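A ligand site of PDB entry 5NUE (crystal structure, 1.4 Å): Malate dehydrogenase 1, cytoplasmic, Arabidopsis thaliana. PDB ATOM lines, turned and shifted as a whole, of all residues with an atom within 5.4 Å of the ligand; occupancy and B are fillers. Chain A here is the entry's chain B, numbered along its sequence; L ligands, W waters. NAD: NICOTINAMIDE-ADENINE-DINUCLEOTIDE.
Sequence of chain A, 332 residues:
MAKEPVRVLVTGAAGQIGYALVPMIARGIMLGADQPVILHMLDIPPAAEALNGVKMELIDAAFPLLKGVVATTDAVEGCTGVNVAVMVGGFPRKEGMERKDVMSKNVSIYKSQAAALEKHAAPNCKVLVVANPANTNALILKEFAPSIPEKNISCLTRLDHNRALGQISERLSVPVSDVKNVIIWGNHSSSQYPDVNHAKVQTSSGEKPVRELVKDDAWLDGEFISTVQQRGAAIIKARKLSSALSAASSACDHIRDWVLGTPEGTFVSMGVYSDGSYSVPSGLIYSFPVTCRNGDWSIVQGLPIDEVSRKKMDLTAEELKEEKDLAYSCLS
The backbone NH (N) of Asn 132 sits at hydrogen-bond distance from an oxygen (O3D) of the ligand (3.0 Å).
An oxygen (O3B) of the ligand is in hydrogen-bond range of the backbone NH (N) of Gly 15 (3.3 Å).
The side-chain carboxylate of Asp 43 is in hydrogen-bond range of an oxygen (O2B) of the ligand (2.6 Å).
The side-chain amide nitrogen of Gln 16 lies within hydrogen-bond range of an oxygen (O1N) of the ligand, 3.4 Å away.
A ring nitrogen (NE2) of His 188 sits at hydrogen-bond distance from a nitrogen (N7N) of the ligand (3.3 Å).
N of Ile 17 is in hydrogen-bond range of O2N of the ligand, at 2.8 Å.
An oxygen (O4B) of the ligand is in hydrogen-bond range of the backbone NH (N) of Gly 90, at 3.2 Å.
An oxygen (O1A) of the ligand is in hydrogen-bond range of the backbone NH of Gln 16 (2.8 Å).
The side-chain amide nitrogen (ND2) of Asn 132 is in hydrogen-bond range of an oxygen (O2D) of the ligand (3.1 Å).
N1A of the ligand lies within hydrogen-bond range of NE2 of Gln 113, at 3.0 Å.
The backbone NH (N) of Gly 12 is in hydrogen-bond range of a nitrogen (N3A) of the ligand, at 3.4 Å.
An oxygen (O3D) of the ligand is in hydrogen-bond range of the backbone carbonyl oxygen (O) of Phe 91.
O of Val 129 is in hydrogen-bond range of N of Leu 156, at 3.0 Å.
The backbone carbonyl oxygen (O) of Leu 42 lies within hydrogen-bond range of the backbone NH (N) of Ala 13 (3.2 Å).
OG1 of Thr 11 lies within hydrogen-bond range of N of Val 88, at 3.0 Å.
The side-chain amide oxygen (OD1) of Asn 132 sits at hydrogen-bond distance from the backbone NH (N) of Ala 134, 3.3 Å away.
N of Ala 14 is in hydrogen-bond range of OD2 of Asp 43 (2.9 Å).
The backbone NH (N) of Phe 91 is in hydrogen-bond range of the side-chain amide oxygen (OD1) of Asn 106 (2.8 Å).
The backbone NH (N) of Gly 89 lies within hydrogen-bond range of the side-chain hydroxyl (OG1) of Thr 11 (3.0 Å).
The backbone NH (N) of Gly 12 lies within hydrogen-bond range of the backbone carbonyl oxygen (O) of Leu 42 (2.9 Å).
An oxygen (O7N) of the ligand sits close to the backbone carbonyl oxygen (O) of Val 130 (3.0 Å).
Ala 14 touches the ligand.
Leu 42 touches the ligand.
CG2 of Ile 44 touches C6A of the ligand, 3.3 Å away.
Val 88 touches the ligand (O to C5D, 3.5 Å).
Gly 89 touches the ligand (CA to O4B, 3.5 Å).
CD of Pro 92 touches O2A of the ligand (3.3 Å).
ND2 of Asn 106 touches O3D of the ligand, at 3.7 Å.
Ile 109 touches the ligand (CD1 to N7A, 3.6 Å).
Ala 131 touches the ligand.
O of Leu 156 touches O7N of the ligand, 3.5 Å away.
Leu 159 touches the ligand.
Ser 242 touches the ligand.
CB of Ala 247 touches C4N of the ligand, at 3.8 Å.
Hydrophobic or aromatic side chains that line the ligand: Ile 17, Ile 44, Val 88, Pro 92, Ile 109, Val 130, Ala 131, Leu 156, Leu 159, His 188 and Ala 247.
Within 4 Å of the ligand: Gly 12, Ala 14, Gly 15, Gln 16, Ile 17, Leu 42, Asp 43, Ile 44, Val 88, Gly 89, Gly 90, Phe 91, Pro 92, Asn 106, Ile 109, Gln 113, Val 130, Ala 131, Asn 132, Leu 156, Leu 159, His 188, Ser 242 and Ala 247.
Water W11 bridges an oxygen (O1N) of the ligand (2.7 Å) and the side-chain amide nitrogen (NE2) of Gln 16 (3.0 Å).
Water W8 lies within hydrogen-bond range of the backbone carbonyl oxygen (O) of Leu 156 (2.8 Å), a nitrogen (N7N) of the ligand (2.8 Å) and the backbone NH (N) of Leu 159 (3.1 Å).
Water W7 lies within hydrogen-bond range of NE2 of Gln 113 (3.0 Å) and N6A of the ligand (3.4 Å).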
ATOM      1  N   THR A  11     -28.692   4.838   8.235  1.00  0.00           N
ATOM      2  CA  THR A  11     -27.368   5.457   8.284  1.00  0.00           C
ATOM      3  C   THR A  11     -26.979   5.665   9.752  1.00  0.00           C
ATOM      4  O   THR A  11     -27.828   5.652  10.644  1.00  0.00           O
ATOM      5  CB  THR A  11     -27.288   6.801   7.526  1.00  0.00           C
ATOM      6  OG1 THR A  11     -27.985   7.803   8.266  1.00  0.00           O
ATOM      7  CG2 THR A  11     -27.914   6.655   6.110  1.00  0.00           C
ATOM      8  N   GLY A  12     -25.672   5.869  10.008  1.00  0.00           N
ATOM      9  CA  GLY A  12     -25.216   5.889  11.394  1.00  0.00           C
ATOM     10  C   GLY A  12     -25.343   4.551  12.064  1.00  0.00           C
ATOM     11  O   GLY A  12     -25.437   4.478  13.283  1.00  0.00           O
ATOM     12  N   ALA A  13     -25.318   3.463  11.279  1.00  0.00           N
ATOM     13  CA  ALA A  13     -25.766   2.172  11.791  1.00  0.00           C
ATOM     14  C   ALA A  13     -24.843   1.572  12.835  1.00  0.00           C
ATOM     15  O   ALA A  13     -25.278   0.695  13.579  1.00  0.00           O
ATOM     16  CB  ALA A  13     -25.945   1.201  10.633  1.00  0.00           C
ATOM     17  N   ALA A  14     -23.556   1.984  12.893  1.00  0.00           N
ATOM     18  CA  ALA A  14     -22.650   1.448  13.907  1.00  0.00           C
ATOM     19  C   ALA A  14     -22.723   2.173  15.252  1.00  0.00           C
ATOM     20  O   ALA A  14     -21.971   1.812  16.169  1.00  0.00           O
ATOM     21  CB  ALA A  14     -21.191   1.451  13.391  1.00  0.00           C
ATOM     22  N   GLY A  15     -23.607   3.170  15.382  1.00  0.00           N
ATOM     23  CA  GLY A  15     -23.720   3.977  16.585  1.00  0.00           C
ATOM     24  C   GLY A  15     -24.798   3.476  17.527  1.00  0.00           C
ATOM     25  O   GLY A  15     -25.373   2.398  17.352  1.00  0.00           O
ATOM     26  N   GLN A  16     -25.022   4.261  18.598  1.00  0.00           N
ATOM     27  CA  GLN A  16     -25.920   3.838  19.670  1.00  0.00           C
ATOM     28  C   GLN A  16     -27.351   3.649  19.181  1.00  0.00           C
ATOM     29  O   GLN A  16     -27.988   2.615  19.446  1.00  0.00           O
ATOM     30  CB  GLN A  16     -25.925   4.872  20.794  1.00  0.00           C
ATOM     31  CG  GLN A  16     -26.415   4.281  22.072  1.00  0.00           C
ATOM     32  CD  GLN A  16     -26.714   5.302  23.169  1.00  0.00           C
ATOM     33  OE1 GLN A  16     -27.049   4.911  24.304  1.00  0.00           O
ATOM     34  NE2 GLN A  16     -26.634   6.591  22.840  1.00  0.00           N
ATOM     35  N   ILE A  17     -27.899   4.644  18.476  1.00  0.00           N
ATOM     36  CA  ILE A  17     -29.279   4.514  17.977  1.00  0.00           C
ATOM     37  C   ILE A  17     -29.364   3.425  16.923  1.00  0.00           C
ATOM     38  O   ILE A  17     -30.299   2.601  16.934  1.00  0.00           O
ATOM     39  CB  ILE A  17     -29.824   5.851  17.467  1.00  0.00           C
ATOM     40  CG1 ILE A  17     -30.015   6.751  18.687  1.00  0.00           C
ATOM     41  CG2 ILE A  17     -31.163   5.635  16.747  1.00  0.00           C
ATOM     42  CD1 ILE A  17     -30.408   8.169  18.252  1.00  0.00           C
ATOM     43  N   GLY A  18     -28.388   3.374  15.998  1.00  0.00           N
ATOM     44  CA  GLY A  18     -28.417   2.325  14.985  1.00  0.00           C
ATOM     45  C   GLY A  18     -28.455   0.942  15.613  1.00  0.00           C
ATOM     46  O   GLY A  18     -29.206   0.064  15.161  1.00  0.00           O
ATOM     47  N   LEU A  42     -25.375   1.941   6.715  1.00  0.00           N
ATOM     48  CA  LEU A  42     -24.332   2.840   6.219  1.00  0.00           C
ATOM     49  C   LEU A  42     -23.649   3.494   7.408  1.00  0.00           C
ATOM     50  O   LEU A  42     -24.318   4.025   8.307  1.00  0.00           O
ATOM     51  CB  LEU A  42     -24.916   3.903   5.310  1.00  0.00           C
ATOM     52  CG  LEU A  42     -23.943   4.926   4.708  1.00  0.00           C
ATOM     53  CD1 LEU A  42     -22.938   4.254   3.703  1.00  0.00           C
ATOM     54  CD2 LEU A  42     -24.682   6.081   4.002  1.00  0.00           C
ATOM     55  N   ASP A  43     -22.322   3.471   7.425  1.00  0.00           N
ATOM     56  CA  ASP A  43     -21.548   4.244   8.401  1.00  0.00           C
ATOM     57  C   ASP A  43     -20.332   4.808   7.673  1.00  0.00           C
ATOM     58  O   ASP A  43     -20.327   4.880   6.427  1.00  0.00           O
ATOM     59  CB  ASP A  43     -21.323   3.429   9.708  1.00  0.00           C
ATOM     60  CG  ASP A  43     -21.189   4.321  10.927  1.00  0.00           C
ATOM     61  OD1 ASP A  43     -20.187   5.092  10.987  1.00  0.00           O
ATOM     62  OD2 ASP A  43     -22.069   4.275  11.821  1.00  0.00           O
ATOM     63  N   ILE A  44     -19.286   5.199   8.402  1.00  0.00           N
ATOM     64  CA  ILE A  44     -18.112   5.788   7.752  1.00  0.00           C
ATOM     65  C   ILE A  44     -16.897   4.923   8.030  1.00  0.00           C
ATOM     66  O   ILE A  44     -16.900   4.076   8.945  1.00  0.00           O
ATOM     67  CB  ILE A  44     -17.864   7.243   8.217  1.00  0.00           C
ATOM     68  CG1 ILE A  44     -17.894   7.330   9.756  1.00  0.00           C
ATOM     69  CG2 ILE A  44     -18.871   8.226   7.502  1.00  0.00           C
ATOM     70  CD1 ILE A  44     -17.502   8.691  10.256  1.00  0.00           C
ATOM     71  N   ALA A  47     -15.470   3.428  11.309  1.00  0.00           N
ATOM     72  CA  ALA A  47     -16.337   2.489  12.010  1.00  0.00           C
ATOM     73  C   ALA A  47     -16.540   1.188  11.229  1.00  0.00           C
ATOM     74  O   ALA A  47     -17.467   0.432  11.518  1.00  0.00           O
ATOM     75  CB  ALA A  47     -17.690   3.169  12.322  1.00  0.00           C
ATOM     76  N   VAL A  88     -29.657   8.368  10.688  1.00  0.00           N
ATOM     77  CA  VAL A  88     -29.155   8.541  12.045  1.00  0.00           C
ATOM     78  C   VAL A  88     -27.702   8.961  12.041  1.00  0.00           C
ATOM     79  O   VAL A  88     -27.167   9.332  13.081  1.00  0.00           O
ATOM     80  CB  VAL A  88     -29.366   7.254  12.869  1.00  0.00           C
ATOM     81  CG1 VAL A  88     -29.151   7.524  14.328  1.00  0.00           C
ATOM     82  CG2 VAL A  88     -30.759   6.654  12.544  1.00  0.00           C
ATOM     83  N   GLY A  89     -27.051   8.973  10.876  1.00  0.00           N
ATOM     84  CA  GLY A  89     -25.625   9.292  10.811  1.00  0.00           C
ATOM     85  C   GLY A  89     -25.362  10.733  11.264  1.00  0.00           C
ATOM     86  O   GLY A  89     -26.063  11.682  10.863  1.00  0.00           O
ATOM     87  N   GLY A  90     -24.395  10.915  12.138  1.00  0.00           N
ATOM     88  CA  GLY A  90     -24.032  12.232  12.655  1.00  0.00           C
ATOM     89  C   GLY A  90     -23.591  12.106  14.103  1.00  0.00           C
ATOM     90  O   GLY A  90     -23.877  11.117  14.788  1.00  0.00           O
ATOM     91  N   PHE A  91     -22.977  13.154  14.588  1.00  0.00           N
ATOM     92  CA  PHE A  91     -22.475  13.214  15.964  1.00  0.00           C
ATOM     93  C   PHE A  91     -23.603  13.542  16.931  1.00  0.00           C
ATOM     94  O   PHE A  91     -24.513  14.308  16.582  1.00  0.00           O
ATOM     95  CB  PHE A  91     -21.460  14.327  16.104  1.00  0.00           C
ATOM     96  CG  PHE A  91     -20.164  14.069  15.409  1.00  0.00           C
ATOM     97  CD1 PHE A  91     -20.035  14.216  14.027  1.00  0.00           C
ATOM     98  CD2 PHE A  91     -19.054  13.672  16.146  1.00  0.00           C
ATOM     99  CE1 PHE A  91     -18.833  13.996  13.406  1.00  0.00           C
ATOM    100  CE2 PHE A  91     -17.824  13.434  15.506  1.00  0.00           C
ATOM    101  CZ  PHE A  91     -17.722  13.598  14.143  1.00  0.00           C
ATOM    102  N   PRO A  92     -23.580  12.913  18.130  1.00  0.00           N
ATOM    103  CA  PRO A  92     -24.519  13.243  19.200  1.00  0.00           C
ATOM    104  C   PRO A  92     -23.986  14.405  20.027  1.00  0.00           C
ATOM    105  O   PRO A  92     -22.801  14.772  19.970  1.00  0.00           O
ATOM    106  CB  PRO A  92     -24.523  11.970  20.067  1.00  0.00           C
ATOM    107  CG  PRO A  92     -23.136  11.479  19.936  1.00  0.00           C
ATOM    108  CD  PRO A  92     -22.682  11.811  18.498  1.00  0.00           C
ATOM    109  N   ARG A  93     -24.877  15.051  20.754  1.00  0.00           N
ATOM    110  CA  ARG A  93     -24.381  16.111  21.616  1.00  0.00           C
ATOM    111  C   ARG A  93     -23.848  15.519  22.919  1.00  0.00           C
ATOM    112  O   ARG A  93     -24.220  14.420  23.332  1.00  0.00           O
ATOM    113  CB  ARG A  93     -25.415  17.214  21.872  1.00  0.00           C
ATOM    114  CG  ARG A  93     -26.732  16.722  22.367  1.00  0.00           C
ATOM    115  CD  ARG A  93     -27.607  17.821  22.980  1.00  0.00           C
ATOM    116  NE  ARG A  93     -28.886  17.225  23.300  1.00  0.00           N
ATOM    117  CZ  ARG A  93     -29.803  17.778  24.087  1.00  0.00           C
ATOM    118  NH1 ARG A  93     -29.567  18.937  24.709  1.00  0.00           N
ATOM    119  NH2 ARG A  93     -30.968  17.156  24.273  1.00  0.00           N
ATOM    120  N   VAL A 102     -24.498  20.260  17.303  1.00  0.00           N
ATOM    121  CA  VAL A 102     -23.900  19.331  16.353  1.00  0.00           C
ATOM    122  C   VAL A 102     -24.177  19.747  14.904  1.00  0.00           C
ATOM    123  O   VAL A 102     -23.839  18.995  13.965  1.00  0.00           O
ATOM    124  CB  VAL A 102     -24.262  17.871  16.655  1.00  0.00           C
ATOM    125  CG1 VAL A 102     -23.673  17.466  18.017  1.00  0.00           C
ATOM    126  CG2 VAL A 102     -25.790  17.708  16.671  1.00  0.00           C
ATOM    127  N   ASN A 106     -22.775  17.988  11.366  1.00  0.00           N
ATOM    128  CA  ASN A 106     -23.737  17.099  10.737  1.00  0.00           C
ATOM    129  C   ASN A 106     -24.355  17.607   9.433  1.00  0.00           C
ATOM    130  O   ASN A 106     -24.755  16.784   8.595  1.00  0.00           O
ATOM    131  CB  ASN A 106     -24.811  16.736  11.756  1.00  0.00           C
ATOM    132  CG  ASN A 106     -24.267  15.875  12.912  1.00  0.00           C
ATOM    133  OD1 ASN A 106     -23.133  15.357  12.852  1.00  0.00           O
ATOM    134  ND2 ASN A 106     -25.082  15.718  13.953  1.00  0.00           N
ATOM    135  N   ILE A 109     -23.177  16.179   6.161  1.00  0.00           N
ATOM    136  CA  ILE A 109     -23.612  14.822   5.873  1.00  0.00           C
ATOM    137  C   ILE A 109     -24.883  14.840   5.043  1.00  0.00           C
ATOM    138  O   ILE A 109     -25.040  14.063   4.092  1.00  0.00           O
ATOM    139  CB  ILE A 109     -23.842  14.046   7.186  1.00  0.00           C
ATOM    140  CG1 ILE A 109     -22.569  13.977   8.037  1.00  0.00           C
ATOM    141  CG2 ILE A 109     -24.434  12.654   6.880  1.00  0.00           C
ATOM    142  CD1 ILE A 109     -22.857  13.374   9.405  1.00  0.00           C
ATOM    143  N   GLN A 113     -25.508  13.340   1.387  1.00  0.00           N
ATOM    144  CA  GLN A 113     -26.340  12.170   1.215  1.00  0.00           C
ATOM    145  C   GLN A 113     -27.654  12.486   0.514  1.00  0.00           C
ATOM    146  O   GLN A 113     -28.290  11.563  -0.035  1.00  0.00           O
ATOM    147  CB  GLN A 113     -26.552  11.452   2.537  1.00  0.00           C
ATOM    148  CG  GLN A 113     -25.247  10.867   3.015  1.00  0.00           C
ATOM    149  CD  GLN A 113     -25.355  10.197   4.352  1.00  0.00           C
ATOM    150  OE1 GLN A 113     -26.382  10.261   4.988  1.00  0.00           O
ATOM    151  NE2 GLN A 113     -24.251   9.619   4.831  1.00  0.00           N
ATOM    152  N   VAL A 129     -35.341  11.727   9.027  1.00  0.00           N
ATOM    153  CA  VAL A 129     -34.084  12.191   9.603  1.00  0.00           C
ATOM    154  C   VAL A 129     -34.191  12.193  11.123  1.00  0.00           C
ATOM    155  O   VAL A 129     -35.084  12.830  11.708  1.00  0.00           O
ATOM    156  CB  VAL A 129     -33.713  13.583   9.085  1.00  0.00           C
ATOM    157  CG1 VAL A 129     -32.389  14.026   9.749  1.00  0.00           C
ATOM    158  CG2 VAL A 129     -33.552  13.497   7.580  1.00  0.00           C
ATOM    159  N   VAL A 130     -33.277  11.455  11.767  1.00  0.00           N
ATOM    160  CA  VAL A 130     -33.187  11.384  13.219  1.00  0.00           C
ATOM    161  C   VAL A 130     -32.051  12.246  13.753  1.00  0.00           C
ATOM    162  O   VAL A 130     -32.187  12.904  14.795  1.00  0.00           O
ATOM    163  CB  VAL A 130     -33.018   9.917  13.654  1.00  0.00           C
ATOM    164  CG1 VAL A 130     -32.774   9.784  15.206  1.00  0.00           C
ATOM    165  CG2 VAL A 130     -34.212   9.054  13.195  1.00  0.00           C
ATOM    166  N   ALA A 131     -30.907  12.210  13.052  1.00  0.00           N
ATOM    167  CA  ALA A 131     -29.721  12.924  13.555  1.00  0.00           C
ATOM    168  C   ALA A 131     -29.989  14.407  13.792  1.00  0.00           C
ATOM    169  O   ALA A 131     -30.670  15.078  13.007  1.00  0.00           O
ATOM    170  CB  ALA A 131     -28.547  12.769  12.568  1.00  0.00           C
ATOM    171  N   ASN A 132     -29.389  14.941  14.888  1.00  0.00           N
ATOM    172  CA  ASN A 132     -29.629  16.341  15.218  1.00  0.00           C
ATOM    173  C   ASN A 132     -28.697  17.272  14.470  1.00  0.00           C
ATOM    174  O   ASN A 132     -27.635  16.858  13.986  1.00  0.00           O
ATOM    175  CB  ASN A 132     -29.446  16.529  16.732  1.00  0.00           C
ATOM    176  CG  ASN A 132     -30.712  16.134  17.475  1.00  0.00           C
ATOM    177  OD1 ASN A 132     -31.799  16.427  16.976  1.00  0.00           O
ATOM    178  ND2 ASN A 132     -30.594  15.415  18.598  1.00  0.00           N
ATOM    179  N   ALA A 134     -32.479  17.762  14.025  1.00  0.00           N
ATOM    180  CA  ALA A 134     -33.250  16.900  13.121  1.00  0.00           C
ATOM    181  C   ALA A 134     -33.988  17.700  12.035  1.00  0.00           C
ATOM    182  O   ALA A 134     -33.908  17.375  10.834  1.00  0.00           O
ATOM    183  CB  ALA A 134     -34.230  16.068  13.941  1.00  0.00           C
ATOM    184  N   LEU A 156     -37.747  13.415  12.946  1.00  0.00           N
ATOM    185  CA  LEU A 156     -38.287  12.715  14.112  1.00  0.00           C
ATOM    186  C   LEU A 156     -38.591  13.708  15.233  1.00  0.00           C
ATOM    187  O   LEU A 156     -37.683  14.142  15.939  1.00  0.00           O
ATOM    188  CB  LEU A 156     -37.279  11.700  14.645  1.00  0.00           C
ATOM    189  CG  LEU A 156     -37.872  10.726  15.680  1.00  0.00           C
ATOM    190  CD1 LEU A 156     -38.847   9.707  15.067  1.00  0.00           C
ATOM    191  CD2 LEU A 156     -36.791   9.990  16.496  1.00  0.00           C
ATOM    192  N   LEU A 159     -40.240  11.061  19.241  1.00  0.00           N
ATOM    193  CA  LEU A 159     -39.755  10.847  20.602  1.00  0.00           C
ATOM    194  C   LEU A 159     -40.247  11.946  21.547  1.00  0.00           C
ATOM    195  O   LEU A 159     -40.655  11.635  22.681  1.00  0.00           O
ATOM    196  CB  LEU A 159     -38.221  10.712  20.629  1.00  0.00           C
ATOM    197  CG  LEU A 159     -37.611  10.552  22.035  1.00  0.00           C
ATOM    198  CD1 LEU A 159     -38.177   9.327  22.805  1.00  0.00           C
ATOM    199  CD2 LEU A 159     -36.089  10.388  21.885  1.00  0.00           C
ATOM    200  N   ARG A 163     -42.542  11.099  24.657  1.00  0.00           N
ATOM    201  CA  ARG A 163     -42.173  11.602  25.989  1.00  0.00           C
ATOM    202  C   ARG A 163     -43.350  12.312  26.637  1.00  0.00           C
ATOM    203  O   ARG A 163     -43.576  12.169  27.866  1.00  0.00           O
ATOM    204  CB  ARG A 163     -41.004  12.588  25.864  1.00  0.00           C
ATOM    205  CG  ARG A 163     -39.635  11.869  25.643  1.00  0.00           C
ATOM    206  CD  ARG A 163     -38.617  12.843  25.091  1.00  0.00           C
ATOM    207  NE  ARG A 163     -37.265  12.247  25.106  1.00  0.00           N
ATOM    208  CZ  ARG A 163     -36.227  12.755  24.444  1.00  0.00           C
ATOM    209  NH1 ARG A 163     -36.380  13.858  23.714  1.00  0.00           N
ATOM    210  NH2 ARG A 163     -35.003  12.173  24.522  1.00  0.00           N
ATOM    211  N   HIS A 188     -37.484  20.256  16.823  1.00  0.00           N
ATOM    212  CA  HIS A 188     -36.977  19.333  17.840  1.00  0.00           C
ATOM    213  C   HIS A 188     -35.886  20.048  18.644  1.00  0.00           C
ATOM    214  O   HIS A 188     -34.678  19.834  18.443  1.00  0.00           O
ATOM    215  CB  HIS A 188     -36.476  18.032  17.166  1.00  0.00           C
ATOM    216  CG  HIS A 188     -35.935  17.014  18.115  1.00  0.00           C
ATOM    217  ND1 HIS A 188     -36.710  16.410  19.085  1.00  0.00           N
ATOM    218  CD2 HIS A 188     -34.687  16.483  18.262  1.00  0.00           C
ATOM    219  CE1 HIS A 188     -35.962  15.573  19.795  1.00  0.00           C
ATOM    220  NE2 HIS A 188     -34.735  15.605  19.329  1.00  0.00           N
ATOM    221  N   SER A 242     -26.741  10.168  25.095  1.00  0.00           N
ATOM    222  CA  SER A 242     -28.093  10.599  24.766  1.00  0.00           C
ATOM    223  C   SER A 242     -28.968   9.381  24.473  1.00  0.00           C
ATOM    224  O   SER A 242     -28.518   8.230  24.479  1.00  0.00           O
ATOM    225  CB  SER A 242     -28.042  11.629  23.663  1.00  0.00           C
ATOM    226  OG  SER A 242     -27.250  11.169  22.585  1.00  0.00           O
ATOM    227  N   SER A 243     -30.464   9.007  24.230  1.00  0.00           N
ATOM    228  CA  SER A 243     -31.728   8.285  24.412  1.00  0.00           C
ATOM    229  C   SER A 243     -31.978   7.302  23.280  1.00  0.00           C
ATOM    230  O   SER A 243     -32.922   7.462  22.512  1.00  0.00           O
ATOM    231  CB  SER A 243     -32.942   9.218  24.377  1.00  0.00           C
ATOM    232  OG  SER A 243     -32.755  10.279  25.226  1.00  0.00           O
ATOM    233  N   ALA A 244     -31.160   6.313  23.175  1.00  0.00           N
ATOM    234  CA  ALA A 244     -31.102   5.488  21.984  1.00  0.00           C
ATOM    235  C   ALA A 244     -32.234   4.471  21.921  1.00  0.00           C
ATOM    236  O   ALA A 244     -32.915   4.332  20.888  1.00  0.00           O
ATOM    237  CB  ALA A 244     -29.728   4.802  21.958  1.00  0.00           C
ATOM    238  N   ALA A 247     -35.276   6.620  21.227  1.00  0.00           N
ATOM    239  CA  ALA A 247     -35.227   7.190  19.871  1.00  0.00           C
ATOM    240  C   ALA A 247     -35.487   6.122  18.815  1.00  0.00           C
ATOM    241  O   ALA A 247     -36.254   6.350  17.870  1.00  0.00           O
ATOM    242  CB  ALA A 247     -33.917   7.926  19.596  1.00  0.00           C
HETATM  243  PA  NAD L   1     -23.380   7.769  17.794  1.00  0.00           P
HETATM  244  O1A NAD L   1     -23.405   6.568  18.739  1.00  0.00           O
HETATM  245  O2A NAD L   1     -22.158   8.644  17.744  1.00  0.00           O
HETATM  246  O5B NAD L   1     -23.718   7.228  16.306  1.00  0.00           O
HETATM  247  C5B NAD L   1     -23.602   8.055  15.188  1.00  0.00           C
HETATM  248  C4B NAD L   1     -23.005   7.158  14.111  1.00  0.00           C
HETATM  249  O4B NAD L   1     -23.080   8.073  12.841  1.00  0.00           O
HETATM  250  C3B NAD L   1     -21.650   6.839  14.268  1.00  0.00           C
HETATM  251  O3B NAD L   1     -21.439   5.388  14.167  1.00  0.00           O
HETATM  252  C2B NAD L   1     -20.901   7.562  13.145  1.00  0.00           C
HETATM  253  O2B NAD L   1     -19.702   6.985  12.727  1.00  0.00           O
HETATM  254  C1B NAD L   1     -22.040   7.658  12.094  1.00  0.00           C
HETATM  255  N9A NAD L   1     -21.640   8.703  11.118  1.00  0.00           N
HETATM  256  C8A NAD L   1     -20.934   9.851  11.117  1.00  0.00           C
HETATM  257  N7A NAD L   1     -20.953  10.332   9.891  1.00  0.00           N
HETATM  258  C5A NAD L   1     -21.683   9.530   9.093  1.00  0.00           C
HETATM  259  C6A NAD L   1     -21.909   9.578   7.729  1.00  0.00           C
HETATM  260  N6A NAD L   1     -21.428  10.608   6.813  1.00  0.00           N
HETATM  261  N1A NAD L   1     -22.672   8.626   7.197  1.00  0.00           N
HETATM  262  C2A NAD L   1     -23.179   7.603   7.957  1.00  0.00           C
HETATM  263  N3A NAD L   1     -22.869   7.550   9.260  1.00  0.00           N
HETATM  264  C4A NAD L   1     -22.123   8.501   9.851  1.00  0.00           C
HETATM  265  O3  NAD L   1     -24.630   8.754  18.121  1.00  0.00           O
HETATM  266  PN  NAD L   1     -26.145   8.312  18.488  1.00  0.00           P
HETATM  267  O1N NAD L   1     -26.255   8.363  19.965  1.00  0.00           O
HETATM  268  O2N NAD L   1     -26.562   7.047  17.773  1.00  0.00           O
HETATM  269  O5D NAD L   1     -26.962   9.599  17.935  1.00  0.00           O
HETATM  270  C5D NAD L   1     -27.087   9.704  16.550  1.00  0.00           C
HETATM  271  C4D NAD L   1     -27.812  11.002  16.190  1.00  0.00           C
HETATM  272  O4D NAD L   1     -29.132  10.978  16.593  1.00  0.00           O
HETATM  273  C3D NAD L   1     -27.159  12.245  16.824  1.00  0.00           C
HETATM  274  O3D NAD L   1     -27.098  13.352  15.999  1.00  0.00           O
HETATM  275  C2D NAD L   1     -28.154  12.410  18.008  1.00  0.00           C
HETATM  276  O2D NAD L   1     -28.033  13.753  18.647  1.00  0.00           O
HETATM  277  C1D NAD L   1     -29.376  12.284  17.367  1.00  0.00           C
HETATM  278  N1N NAD L   1     -30.531  11.991  18.207  1.00  0.00           N
HETATM  279  C2N NAD L   1     -31.747  12.351  17.750  1.00  0.00           C
HETATM  280  C3N NAD L   1     -32.903  12.144  18.487  1.00  0.00           C
HETATM  281  C7N NAD L   1     -34.241  12.607  17.905  1.00  0.00           C
HETATM  282  O7N NAD L   1     -34.419  13.135  16.799  1.00  0.00           O
HETATM  283  N7N NAD L   1     -35.306  12.410  18.811  1.00  0.00           N
HETATM  284  C4N NAD L   1     -32.799  11.560  19.724  1.00  0.00           C
HETATM  285  C5N NAD L   1     -31.580  11.150  20.202  1.00  0.00           C
HETATM  286  C6N NAD L   1     -30.425  11.377  19.451  1.00  0.00           C
HETATM  287  O   HOH W   1     -19.071  12.463   9.581  1.00  0.00           O
HETATM  288  O   HOH W   2     -26.495   5.387  15.659  1.00  0.00           O
HETATM  289  O   HOH W   3     -19.172  12.352   7.184  1.00  0.00           O
HETATM  290  O   HOH W   4     -20.467   8.873  19.829  1.00  0.00           O
HETATM  291  O   HOH W   5     -20.268   9.632  16.398  1.00  0.00           O
HETATM  292  O   HOH W   6     -19.495   4.766  15.999  1.00  0.00           O
HETATM  293  O   HOH W   7     -21.459   9.378   3.666  1.00  0.00           O
HETATM  294  O   HOH W   8     -38.044  13.100  18.532  1.00  0.00           O
HETATM  295  O   HOH W   9     -17.277   7.332  13.974  1.00  0.00           O
HETATM  296  O   HOH W  10     -19.823  10.815  14.072  1.00  0.00           O
HETATM  297  O   HOH W  11     -24.617   8.724  22.126  1.00  0.00           O
HETATM  298  O   HOH W  12     -21.154   5.111  19.038  1.00  0.00           O
